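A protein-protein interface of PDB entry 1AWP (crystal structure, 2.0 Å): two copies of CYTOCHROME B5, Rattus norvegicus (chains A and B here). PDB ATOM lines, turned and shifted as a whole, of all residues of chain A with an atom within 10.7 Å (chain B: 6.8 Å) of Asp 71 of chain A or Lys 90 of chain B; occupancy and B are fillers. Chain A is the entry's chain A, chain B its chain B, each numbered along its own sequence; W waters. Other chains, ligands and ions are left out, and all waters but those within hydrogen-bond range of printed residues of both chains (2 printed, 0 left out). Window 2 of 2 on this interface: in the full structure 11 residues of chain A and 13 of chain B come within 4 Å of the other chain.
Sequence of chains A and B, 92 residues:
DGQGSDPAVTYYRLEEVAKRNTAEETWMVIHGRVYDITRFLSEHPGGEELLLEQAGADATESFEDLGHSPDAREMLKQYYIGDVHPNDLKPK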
ATOM      1  N   PHE A  40      21.390 -28.982  -5.916  1.00  0.00           N
ATOM      2  CA  PHE A  40      21.208 -27.555  -5.687  1.00  0.00           C
ATOM      3  C   PHE A  40      22.436 -26.897  -5.048  1.00  0.00           C
ATOM      4  O   PHE A  40      22.593 -25.678  -5.095  1.00  0.00           O
ATOM      5  CB  PHE A  40      19.976 -27.355  -4.796  1.00  0.00           C
ATOM      6  CG  PHE A  40      19.700 -25.927  -4.439  1.00  0.00           C
ATOM      7  CD1 PHE A  40      19.289 -25.019  -5.410  1.00  0.00           C
ATOM      8  CD2 PHE A  40      19.820 -25.496  -3.123  1.00  0.00           C
ATOM      9  CE1 PHE A  40      19.001 -23.701  -5.074  1.00  0.00           C
ATOM     10  CE2 PHE A  40      19.534 -24.181  -2.778  1.00  0.00           C
ATOM     11  CZ  PHE A  40      19.122 -23.282  -3.755  1.00  0.00           C
ATOM     12  N   HIS A  44      22.867 -22.539  -5.060  1.00  0.00           N
ATOM     13  CA  HIS A  44      22.480 -21.742  -3.905  1.00  0.00           C
ATOM     14  C   HIS A  44      23.174 -20.393  -3.814  1.00  0.00           C
ATOM     15  O   HIS A  44      24.385 -20.311  -3.642  1.00  0.00           O
ATOM     16  CB  HIS A  44      22.739 -22.527  -2.622  1.00  0.00           C
ATOM     17  CG  HIS A  44      22.279 -21.826  -1.385  1.00  0.00           C
ATOM     18  ND1 HIS A  44      23.061 -21.723  -0.254  1.00  0.00           N
ATOM     19  CD2 HIS A  44      21.109 -21.208  -1.093  1.00  0.00           C
ATOM     20  CE1 HIS A  44      22.393 -21.075   0.681  1.00  0.00           C
ATOM     21  NE2 HIS A  44      21.206 -20.751   0.198  1.00  0.00           N
ATOM     22  N   PRO A  45      22.406 -19.314  -3.926  1.00  0.00           N
ATOM     23  CA  PRO A  45      22.954 -17.959  -3.851  1.00  0.00           C
ATOM     24  C   PRO A  45      23.761 -17.691  -2.582  1.00  0.00           C
ATOM     25  O   PRO A  45      24.658 -16.847  -2.577  1.00  0.00           O
ATOM     26  CB  PRO A  45      21.713 -17.071  -3.940  1.00  0.00           C
ATOM     27  CG  PRO A  45      20.718 -17.913  -4.668  1.00  0.00           C
ATOM     28  CD  PRO A  45      20.957 -19.307  -4.171  1.00  0.00           C
ATOM     29  N   PHE A  63      17.122 -21.664   8.062  1.00  0.00           N
ATOM     30  CA  PHE A  63      16.407 -21.291   6.849  1.00  0.00           C
ATOM     31  C   PHE A  63      15.468 -20.131   7.134  1.00  0.00           C
ATOM     32  O   PHE A  63      15.463 -19.123   6.424  1.00  0.00           O
ATOM     33  CB  PHE A  63      15.608 -22.488   6.310  1.00  0.00           C
ATOM     34  CG  PHE A  63      14.810 -22.183   5.067  1.00  0.00           C
ATOM     35  CD1 PHE A  63      15.377 -22.334   3.808  1.00  0.00           C
ATOM     36  CD2 PHE A  63      13.495 -21.743   5.161  1.00  0.00           C
ATOM     37  CE1 PHE A  63      14.642 -22.048   2.653  1.00  0.00           C
ATOM     38  CE2 PHE A  63      12.753 -21.453   4.012  1.00  0.00           C
ATOM     39  CZ  PHE A  63      13.329 -21.605   2.754  1.00  0.00           C
ATOM     40  N   GLY A  67      15.404 -15.373   6.760  1.00  0.00           N
ATOM     41  CA  GLY A  67      14.315 -14.741   6.063  1.00  0.00           C
ATOM     42  C   GLY A  67      14.378 -15.057   4.576  1.00  0.00           C
ATOM     43  O   GLY A  67      14.630 -14.168   3.756  1.00  0.00           O
ATOM     44  N   HIS A  68      14.186 -16.322   4.208  1.00  0.00           N
ATOM     45  CA  HIS A  68      14.206 -16.658   2.797  1.00  0.00           C
ATOM     46  C   HIS A  68      12.931 -16.125   2.135  1.00  0.00           C
ATOM     47  O   HIS A  68      11.881 -16.033   2.768  1.00  0.00           O
ATOM     48  CB  HIS A  68      14.342 -18.161   2.593  1.00  0.00           C
ATOM     49  CG  HIS A  68      15.742 -18.654   2.762  1.00  0.00           C
ATOM     50  ND1 HIS A  68      16.290 -18.913   3.998  1.00  0.00           N
ATOM     51  CD2 HIS A  68      16.717 -18.912   1.855  1.00  0.00           C
ATOM     52  CE1 HIS A  68      17.541 -19.313   3.850  1.00  0.00           C
ATOM     53  NE2 HIS A  68      17.823 -19.320   2.558  1.00  0.00           N
ATOM     54  N   SER A  69      13.033 -15.779   0.857  1.00  0.00           N
ATOM     55  CA  SER A  69      11.918 -15.218   0.112  1.00  0.00           C
ATOM     56  C   SER A  69      10.892 -16.247  -0.324  1.00  0.00           C
ATOM     57  O   SER A  69      11.133 -17.456  -0.252  1.00  0.00           O
ATOM     58  CB  SER A  69      12.446 -14.496  -1.129  1.00  0.00           C
ATOM     59  OG  SER A  69      12.777 -15.433  -2.146  1.00  0.00           O
ATOM     60  N   PRO A  70       9.714 -15.774  -0.763  1.00  0.00           N
ATOM     61  CA  PRO A  70       8.663 -16.684  -1.222  1.00  0.00           C
ATOM     62  C   PRO A  70       9.162 -17.501  -2.415  1.00  0.00           C
ATOM     63  O   PRO A  70       8.698 -18.615  -2.652  1.00  0.00           O
ATOM     64  CB  PRO A  70       7.509 -15.746  -1.600  1.00  0.00           C
ATOM     65  CG  PRO A  70       7.780 -14.482  -0.849  1.00  0.00           C
ATOM     66  CD  PRO A  70       9.276 -14.366  -0.805  1.00  0.00           C
ATOM     67  N   ASP A  71      10.107 -16.937  -3.166  1.00  0.00           N
ATOM     68  CA  ASP A  71      10.678 -17.619  -4.325  1.00  0.00           C
ATOM     69  C   ASP A  71      11.609 -18.736  -3.879  1.00  0.00           C
ATOM     70  O   ASP A  71      11.751 -19.758  -4.557  1.00  0.00           O
ATOM     71  CB  ASP A  71      11.443 -16.635  -5.200  1.00  0.00           C
ATOM     72  CG  ASP A  71      10.542 -15.575  -5.796  1.00  0.00           C
ATOM     73  OD1 ASP A  71       9.575 -15.939  -6.506  1.00  0.00           O
ATOM     74  OD2 ASP A  71      10.796 -14.378  -5.546  1.00  0.00           O
ATOM     75  N   ALA A  72      12.249 -18.535  -2.736  1.00  0.00           N
ATOM     76  CA  ALA A  72      13.137 -19.542  -2.188  1.00  0.00           C
ATOM     77  C   ALA A  72      12.276 -20.723  -1.712  1.00  0.00           C
ATOM     78  O   ALA A  72      12.643 -21.887  -1.909  1.00  0.00           O
ATOM     79  CB  ALA A  72      13.930 -18.954  -1.025  1.00  0.00           C
ATOM     80  N   ARG A  73      11.132 -20.420  -1.091  1.00  0.00           N
ATOM     81  CA  ARG A  73      10.221 -21.463  -0.610  1.00  0.00           C
ATOM     82  C   ARG A  73       9.678 -22.304  -1.762  1.00  0.00           C
ATOM     83  O   ARG A  73       9.504 -23.511  -1.631  1.00  0.00           O
ATOM     84  CB  ARG A  73       9.045 -20.848   0.137  1.00  0.00           C
ATOM     85  CG  ARG A  73       9.387 -20.376   1.522  1.00  0.00           C
ATOM     86  CD  ARG A  73       8.196 -19.711   2.177  1.00  0.00           C
ATOM     87  NE  ARG A  73       8.603 -18.817   3.256  1.00  0.00           N
ATOM     88  CZ  ARG A  73       8.971 -19.229   4.464  1.00  0.00           C
ATOM     89  NH1 ARG A  73       8.986 -20.523   4.754  1.00  0.00           N
ATOM     90  NH2 ARG A  73       9.323 -18.346   5.387  1.00  0.00           N
ATOM     91  N   GLU A  74       9.404 -21.659  -2.889  1.00  0.00           N
ATOM     92  CA  GLU A  74       8.886 -22.362  -4.054  1.00  0.00           C
ATOM     93  C   GLU A  74       9.898 -23.350  -4.610  1.00  0.00           C
ATOM     94  O   GLU A  74       9.536 -24.440  -5.037  1.00  0.00           O
ATOM     95  CB  GLU A  74       8.494 -21.358  -5.140  1.00  0.00           C
ATOM     96  CG  GLU A  74       7.158 -20.685  -4.880  1.00  0.00           C
ATOM     97  CD  GLU A  74       6.067 -21.165  -5.826  1.00  0.00           C
ATOM     98  OE1 GLU A  74       6.100 -22.347  -6.251  1.00  0.00           O
ATOM     99  OE2 GLU A  74       5.175 -20.348  -6.142  1.00  0.00           O
ATOM    100  N   MET A  75      11.168 -22.962  -4.602  1.00  0.00           N
ATOM    101  CA  MET A  75      12.235 -23.815  -5.105  1.00  0.00           C
ATOM    102  C   MET A  75      12.327 -25.131  -4.346  1.00  0.00           C
ATOM    103  O   MET A  75      12.769 -26.139  -4.907  1.00  0.00           O
ATOM    104  CB  MET A  75      13.579 -23.103  -5.004  1.00  0.00           C
ATOM    105  CG  MET A  75      13.684 -21.846  -5.820  1.00  0.00           C
ATOM    106  SD  MET A  75      15.412 -21.389  -5.947  1.00  0.00           S
ATOM    107  CE  MET A  75      16.062 -22.861  -6.824  1.00  0.00           C
ATOM    108  N   LEU A  76      11.923 -25.121  -3.075  1.00  0.00           N
ATOM    109  CA  LEU A  76      11.971 -26.328  -2.245  1.00  0.00           C
ATOM    110  C   LEU A  76      11.178 -27.486  -2.856  1.00  0.00           C
ATOM    111  O   LEU A  76      11.587 -28.650  -2.790  1.00  0.00           O
ATOM    112  CB  LEU A  76      11.417 -26.034  -0.854  1.00  0.00           C
ATOM    113  CG  LEU A  76      12.382 -25.536   0.216  1.00  0.00           C
ATOM    114  CD1 LEU A  76      11.614 -25.316   1.506  1.00  0.00           C
ATOM    115  CD2 LEU A  76      13.493 -26.551   0.417  1.00  0.00           C
ATOM    116  N   LYS A  77      10.044 -27.157  -3.460  1.00  0.00           N
ATOM    117  CA  LYS A  77       9.191 -28.161  -4.052  1.00  0.00           C
ATOM    118  C   LYS A  77       9.882 -29.154  -4.976  1.00  0.00           C
ATOM    119  O   LYS A  77       9.448 -30.302  -5.062  1.00  0.00           O
ATOM    120  CB  LYS A  77       8.038 -27.489  -4.790  1.00  0.00           C
ATOM    121  CG  LYS A  77       6.728 -27.563  -4.036  1.00  0.00           C
ATOM    122  CD  LYS A  77       6.108 -26.188  -3.850  1.00  0.00           C
ATOM    123  CE  LYS A  77       5.454 -25.710  -5.129  1.00  0.00           C
ATOM    124  NZ  LYS A  77       4.443 -24.669  -4.838  1.00  0.00           N
ATOM    125  N   GLN A  78      10.944 -28.753  -5.670  1.00  0.00           N
ATOM    126  CA  GLN A  78      11.591 -29.709  -6.566  1.00  0.00           C
ATOM    127  C   GLN A  78      12.575 -30.659  -5.891  1.00  0.00           C
ATOM    128  O   GLN A  78      13.091 -31.578  -6.534  1.00  0.00           O
ATOM    129  CB  GLN A  78      12.306 -29.005  -7.719  1.00  0.00           C
ATOM    130  CG  GLN A  78      12.440 -27.511  -7.589  1.00  0.00           C
ATOM    131  CD  GLN A  78      13.366 -26.951  -8.648  1.00  0.00           C
ATOM    132  OE1 GLN A  78      13.857 -27.694  -9.506  1.00  0.00           O
ATOM    133  NE2 GLN A  78      13.614 -25.642  -8.599  1.00  0.00           N
ATOM    134  N   TYR A  79      12.828 -30.457  -4.601  1.00  0.00           N
ATOM    135  CA  TYR A  79      13.770 -31.314  -3.892  1.00  0.00           C
ATOM    136  C   TYR A  79      13.098 -32.212  -2.862  1.00  0.00           C
ATOM    137  O   TYR A  79      13.745 -33.053  -2.234  1.00  0.00           O
ATOM    138  CB  TYR A  79      14.847 -30.444  -3.240  1.00  0.00           C
ATOM    139  CG  TYR A  79      15.536 -29.561  -4.248  1.00  0.00           C
ATOM    140  CD1 TYR A  79      16.331 -30.115  -5.260  1.00  0.00           C
ATOM    141  CD2 TYR A  79      15.347 -28.183  -4.236  1.00  0.00           C
ATOM    142  CE1 TYR A  79      16.915 -29.320  -6.236  1.00  0.00           C
ATOM    143  CE2 TYR A  79      15.930 -27.372  -5.212  1.00  0.00           C
ATOM    144  CZ  TYR A  79      16.708 -27.948  -6.207  1.00  0.00           C
ATOM    145  OH  TYR A  79      17.267 -27.146  -7.172  1.00  0.00           O
ATOM    146  N   LEU B  14       4.347 -16.743   5.885  1.00  0.00           N
ATOM    147  CA  LEU B  14       4.503 -18.032   5.224  1.00  0.00           C
ATOM    148  C   LEU B  14       5.196 -19.040   6.125  1.00  0.00           C
ATOM    149  O   LEU B  14       5.061 -20.254   5.947  1.00  0.00           O
ATOM    150  CB  LEU B  14       5.258 -17.869   3.904  1.00  0.00           C
ATOM    151  CG  LEU B  14       4.474 -17.173   2.774  1.00  0.00           C
ATOM    152  CD1 LEU B  14       5.387 -17.012   1.572  1.00  0.00           C
ATOM    153  CD2 LEU B  14       3.234 -17.966   2.389  1.00  0.00           C
ATOM    154  N   ASP B  58       2.608 -22.541  -1.483  1.00  0.00           N
ATOM    155  CA  ASP B  58       1.855 -21.747  -2.446  1.00  0.00           C
ATOM    156  C   ASP B  58       1.604 -22.666  -3.634  1.00  0.00           C
ATOM    157  O   ASP B  58       2.520 -22.965  -4.393  1.00  0.00           O
ATOM    158  CB  ASP B  58       2.683 -20.537  -2.895  1.00  0.00           C
ATOM    159  CG  ASP B  58       1.881 -19.544  -3.723  1.00  0.00           C
ATOM    160  OD1 ASP B  58       0.963 -19.963  -4.453  1.00  0.00           O
ATOM    161  OD2 ASP B  58       2.170 -18.336  -3.649  1.00  0.00           O
ATOM    162  N   THR B  60      -0.552 -21.985  -6.116  1.00  0.00           N
ATOM    163  CA  THR B  60      -1.219 -21.182  -7.138  1.00  0.00           C
ATOM    164  C   THR B  60      -0.926 -21.640  -8.554  1.00  0.00           C
ATOM    165  O   THR B  60      -1.829 -21.755  -9.383  1.00  0.00           O
ATOM    166  CB  THR B  60      -0.813 -19.697  -7.035  1.00  0.00           C
ATOM    167  OG1 THR B  60      -1.176 -19.187  -5.746  1.00  0.00           O
ATOM    168  CG2 THR B  60      -1.517 -18.877  -8.115  1.00  0.00           C
ATOM    169  N   PRO B  86       1.697  -9.010   4.221  1.00  0.00           N
ATOM    170  CA  PRO B  86       2.294  -8.114   3.226  1.00  0.00           C
ATOM    171  C   PRO B  86       3.795  -8.312   3.035  1.00  0.00           C
ATOM    172  O   PRO B  86       4.303  -8.167   1.924  1.00  0.00           O
ATOM    173  CB  PRO B  86       1.955  -6.724   3.757  1.00  0.00           C
ATOM    174  CG  PRO B  86       0.679  -6.923   4.472  1.00  0.00           C
ATOM    175  CD  PRO B  86       0.811  -8.270   5.137  1.00  0.00           C
ATOM    176  N   ASN B  87       4.494  -8.653   4.115  1.00  0.00           N
ATOM    177  CA  ASN B  87       5.936  -8.870   4.062  1.00  0.00           C
ATOM    178  C   ASN B  87       6.321 -10.062   3.206  1.00  0.00           C
ATOM    179  O   ASN B  87       7.426 -10.109   2.683  1.00  0.00           O
ATOM    180  CB  ASN B  87       6.496  -9.083   5.465  1.00  0.00           C
ATOM    181  CG  ASN B  87       6.677  -7.788   6.222  1.00  0.00           C
ATOM    182  OD1 ASN B  87       6.595  -7.758   7.453  1.00  0.00           O
ATOM    183  ND2 ASN B  87       6.923  -6.704   5.493  1.00  0.00           N
ATOM    184  N   ASP B  88       5.416 -11.028   3.062  1.00  0.00           N
ATOM    185  CA  ASP B  88       5.708 -12.221   2.272  1.00  0.00           C
ATOM    186  C   ASP B  88       5.089 -12.238   0.882  1.00  0.00           C
ATOM    187  O   ASP B  88       5.062 -13.286   0.243  1.00  0.00           O
ATOM    188  CB  ASP B  88       5.259 -13.480   3.019  1.00  0.00           C
ATOM    189  CG  ASP B  88       6.082 -13.746   4.255  1.00  0.00           C
ATOM    190  OD1 ASP B  88       7.307 -13.509   4.221  1.00  0.00           O
ATOM    191  OD2 ASP B  88       5.500 -14.189   5.263  1.00  0.00           O
ATOM    192  N   LEU B  89       4.581 -11.100   0.415  1.00  0.00           N
ATOM    193  CA  LEU B  89       3.983 -11.037  -0.917  1.00  0.00           C
ATOM    194  C   LEU B  89       5.090 -10.825  -1.947  1.00  0.00           C
ATOM    195  O   LEU B  89       6.118 -10.229  -1.630  1.00  0.00           O
ATOM    196  CB  LEU B  89       2.980  -9.889  -0.994  1.00  0.00           C
ATOM    197  CG  LEU B  89       1.720 -10.031  -0.143  1.00  0.00           C
ATOM    198  CD1 LEU B  89       0.998  -8.683  -0.048  1.00  0.00           C
ATOM    199  CD2 LEU B  89       0.821 -11.080  -0.762  1.00  0.00           C
ATOM    200  N   LYS B  90       4.888 -11.308  -3.173  1.00  0.00           N
ATOM    201  CA  LYS B  90       5.896 -11.158  -4.230  1.00  0.00           C
ATOM    202  C   LYS B  90       5.534 -10.052  -5.231  1.00  0.00           C
ATOM    203  O   LYS B  90       4.858 -10.306  -6.230  1.00  0.00           O
ATOM    204  CB  LYS B  90       6.083 -12.485  -4.976  1.00  0.00           C
ATOM    205  CG  LYS B  90       5.278 -13.652  -4.404  1.00  0.00           C
ATOM    206  CD  LYS B  90       4.958 -14.685  -5.477  1.00  0.00           C
ATOM    207  CE  LYS B  90       5.872 -15.900  -5.380  1.00  0.00           C
ATOM    208  NZ  LYS B  90       5.110 -17.164  -5.183  1.00  0.00           N
ATOM    209  N   PRO B  91       6.003  -8.813  -4.983  1.00  0.00           N
ATOM    210  CA  PRO B  91       5.736  -7.650  -5.845  1.00  0.00           C
ATOM    211  C   PRO B  91       5.828  -7.916  -7.343  1.00  0.00           C
ATOM    212  O   PRO B  91       5.575  -7.021  -8.151  1.00  0.00           O
ATOM    213  CB  PRO B  91       6.764  -6.619  -5.386  1.00  0.00           C
ATOM    214  CG  PRO B  91       7.001  -6.954  -3.951  1.00  0.00           C
ATOM    215  CD  PRO B  91       6.861  -8.453  -3.836  1.00  0.00           C
HETATM  216  O   HOH W   1       7.470 -16.006   6.802  1.00  0.00           O
HETATM  217  O   HOH W   2       2.765 -21.730  -6.984  1.00  0.00           O
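No position is printed for both chains.
Water W2 lies within hydrogen-bond range of O of Asp 58 of chain B (2.9 Å), OE2 of Glu 74 of chain A (2.9 Å) and N of Thr 60 of chain B (3.4 Å).
Water W1 lies within hydrogen-bond range of the side-chain carboxylate (OD2) of Asp 88 of chain B, the guanidinium group (NH2) of Arg 73 of chain A and the backbone NH (N) of Leu 14 of chain B.
OG of Ser 69 of chain A lies close to N of Asp 71 of chain A (3.2 Å).
OE1 of Glu 74 of chain A is in salt-bridge range of NZ of Lys 77 of chain A (3.2 Å).
The backbone NH (N) of Leu 14 of chain B lies within hydrogen-bond range of the side-chain carboxylate (OD2) of Asp 88 of chain B, at 2.9 Å.
The side-chain carboxylate (OD1) of Asp 58 of chain B sits at hydrogen-bond distance from the side-chain hydroxyl (OG1) of Thr 60 of chain B.
OD2 of Asp 58 of chain B is in salt-bridge range of NZ of Lys 90 of chain B (3.5 Å).
Among the printed residues, merely in contact across the chains: Pro 70 of chain A with Asp 88 of chain B (3.2 Å), Arg 73 of chain A with Leu 14 of chain B (3.5 Å) and Asp 71 of chain A with Lys 90 of chain B (3.9 Å).
Lys 90 of chain B touches just these residues of chain A: Asp 71 (3.9 Å) and Glu 74 (3.3 Å).
No residue of chain A comes within 4 Å of Leu 89 of chain B.
Pro 91 of chain B touches none of the printed residues of chain A.
Of the printed residues of chain A, Asp 88 of chain B touches Pro 70 (3.2 Å).
Printed residues of chain B within 4 Å of Glu 74 of chain A: Lys 90 (3.3 Å).
Of the printed residues of chain A, Leu 14 of chain B touches Arg 73.
His 44 of chain A touches none of the printed residues of chain B.
The nearest residue of chain A that does not touch Lys 90 of chain B is Pro 70 of chain A (4.1 Å).
Of the 17 printed residues of chain A, 5 touch a printed residue of chain B.
Hydrophobic or aromatic side chains of chain B that line the printed part of chain A: Leu 14.
Among the printed residues, Asp or Glu carboxylates within 4 Å of a Lys or Arg side-chain nitrogen of the other chain: Glu 74 of chain A with Lys 90 of chain B.
OE2 of Glu 74 of chain A lies within salt-bridge range of NZ of Lys 90 of chain B.
The side-chain amino group (NZ) of Lys 77 of chain A lies within hydrogen-bond range of the backbone carbonyl oxygen (O) of Asp 58 of chain B (2.6 Å).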
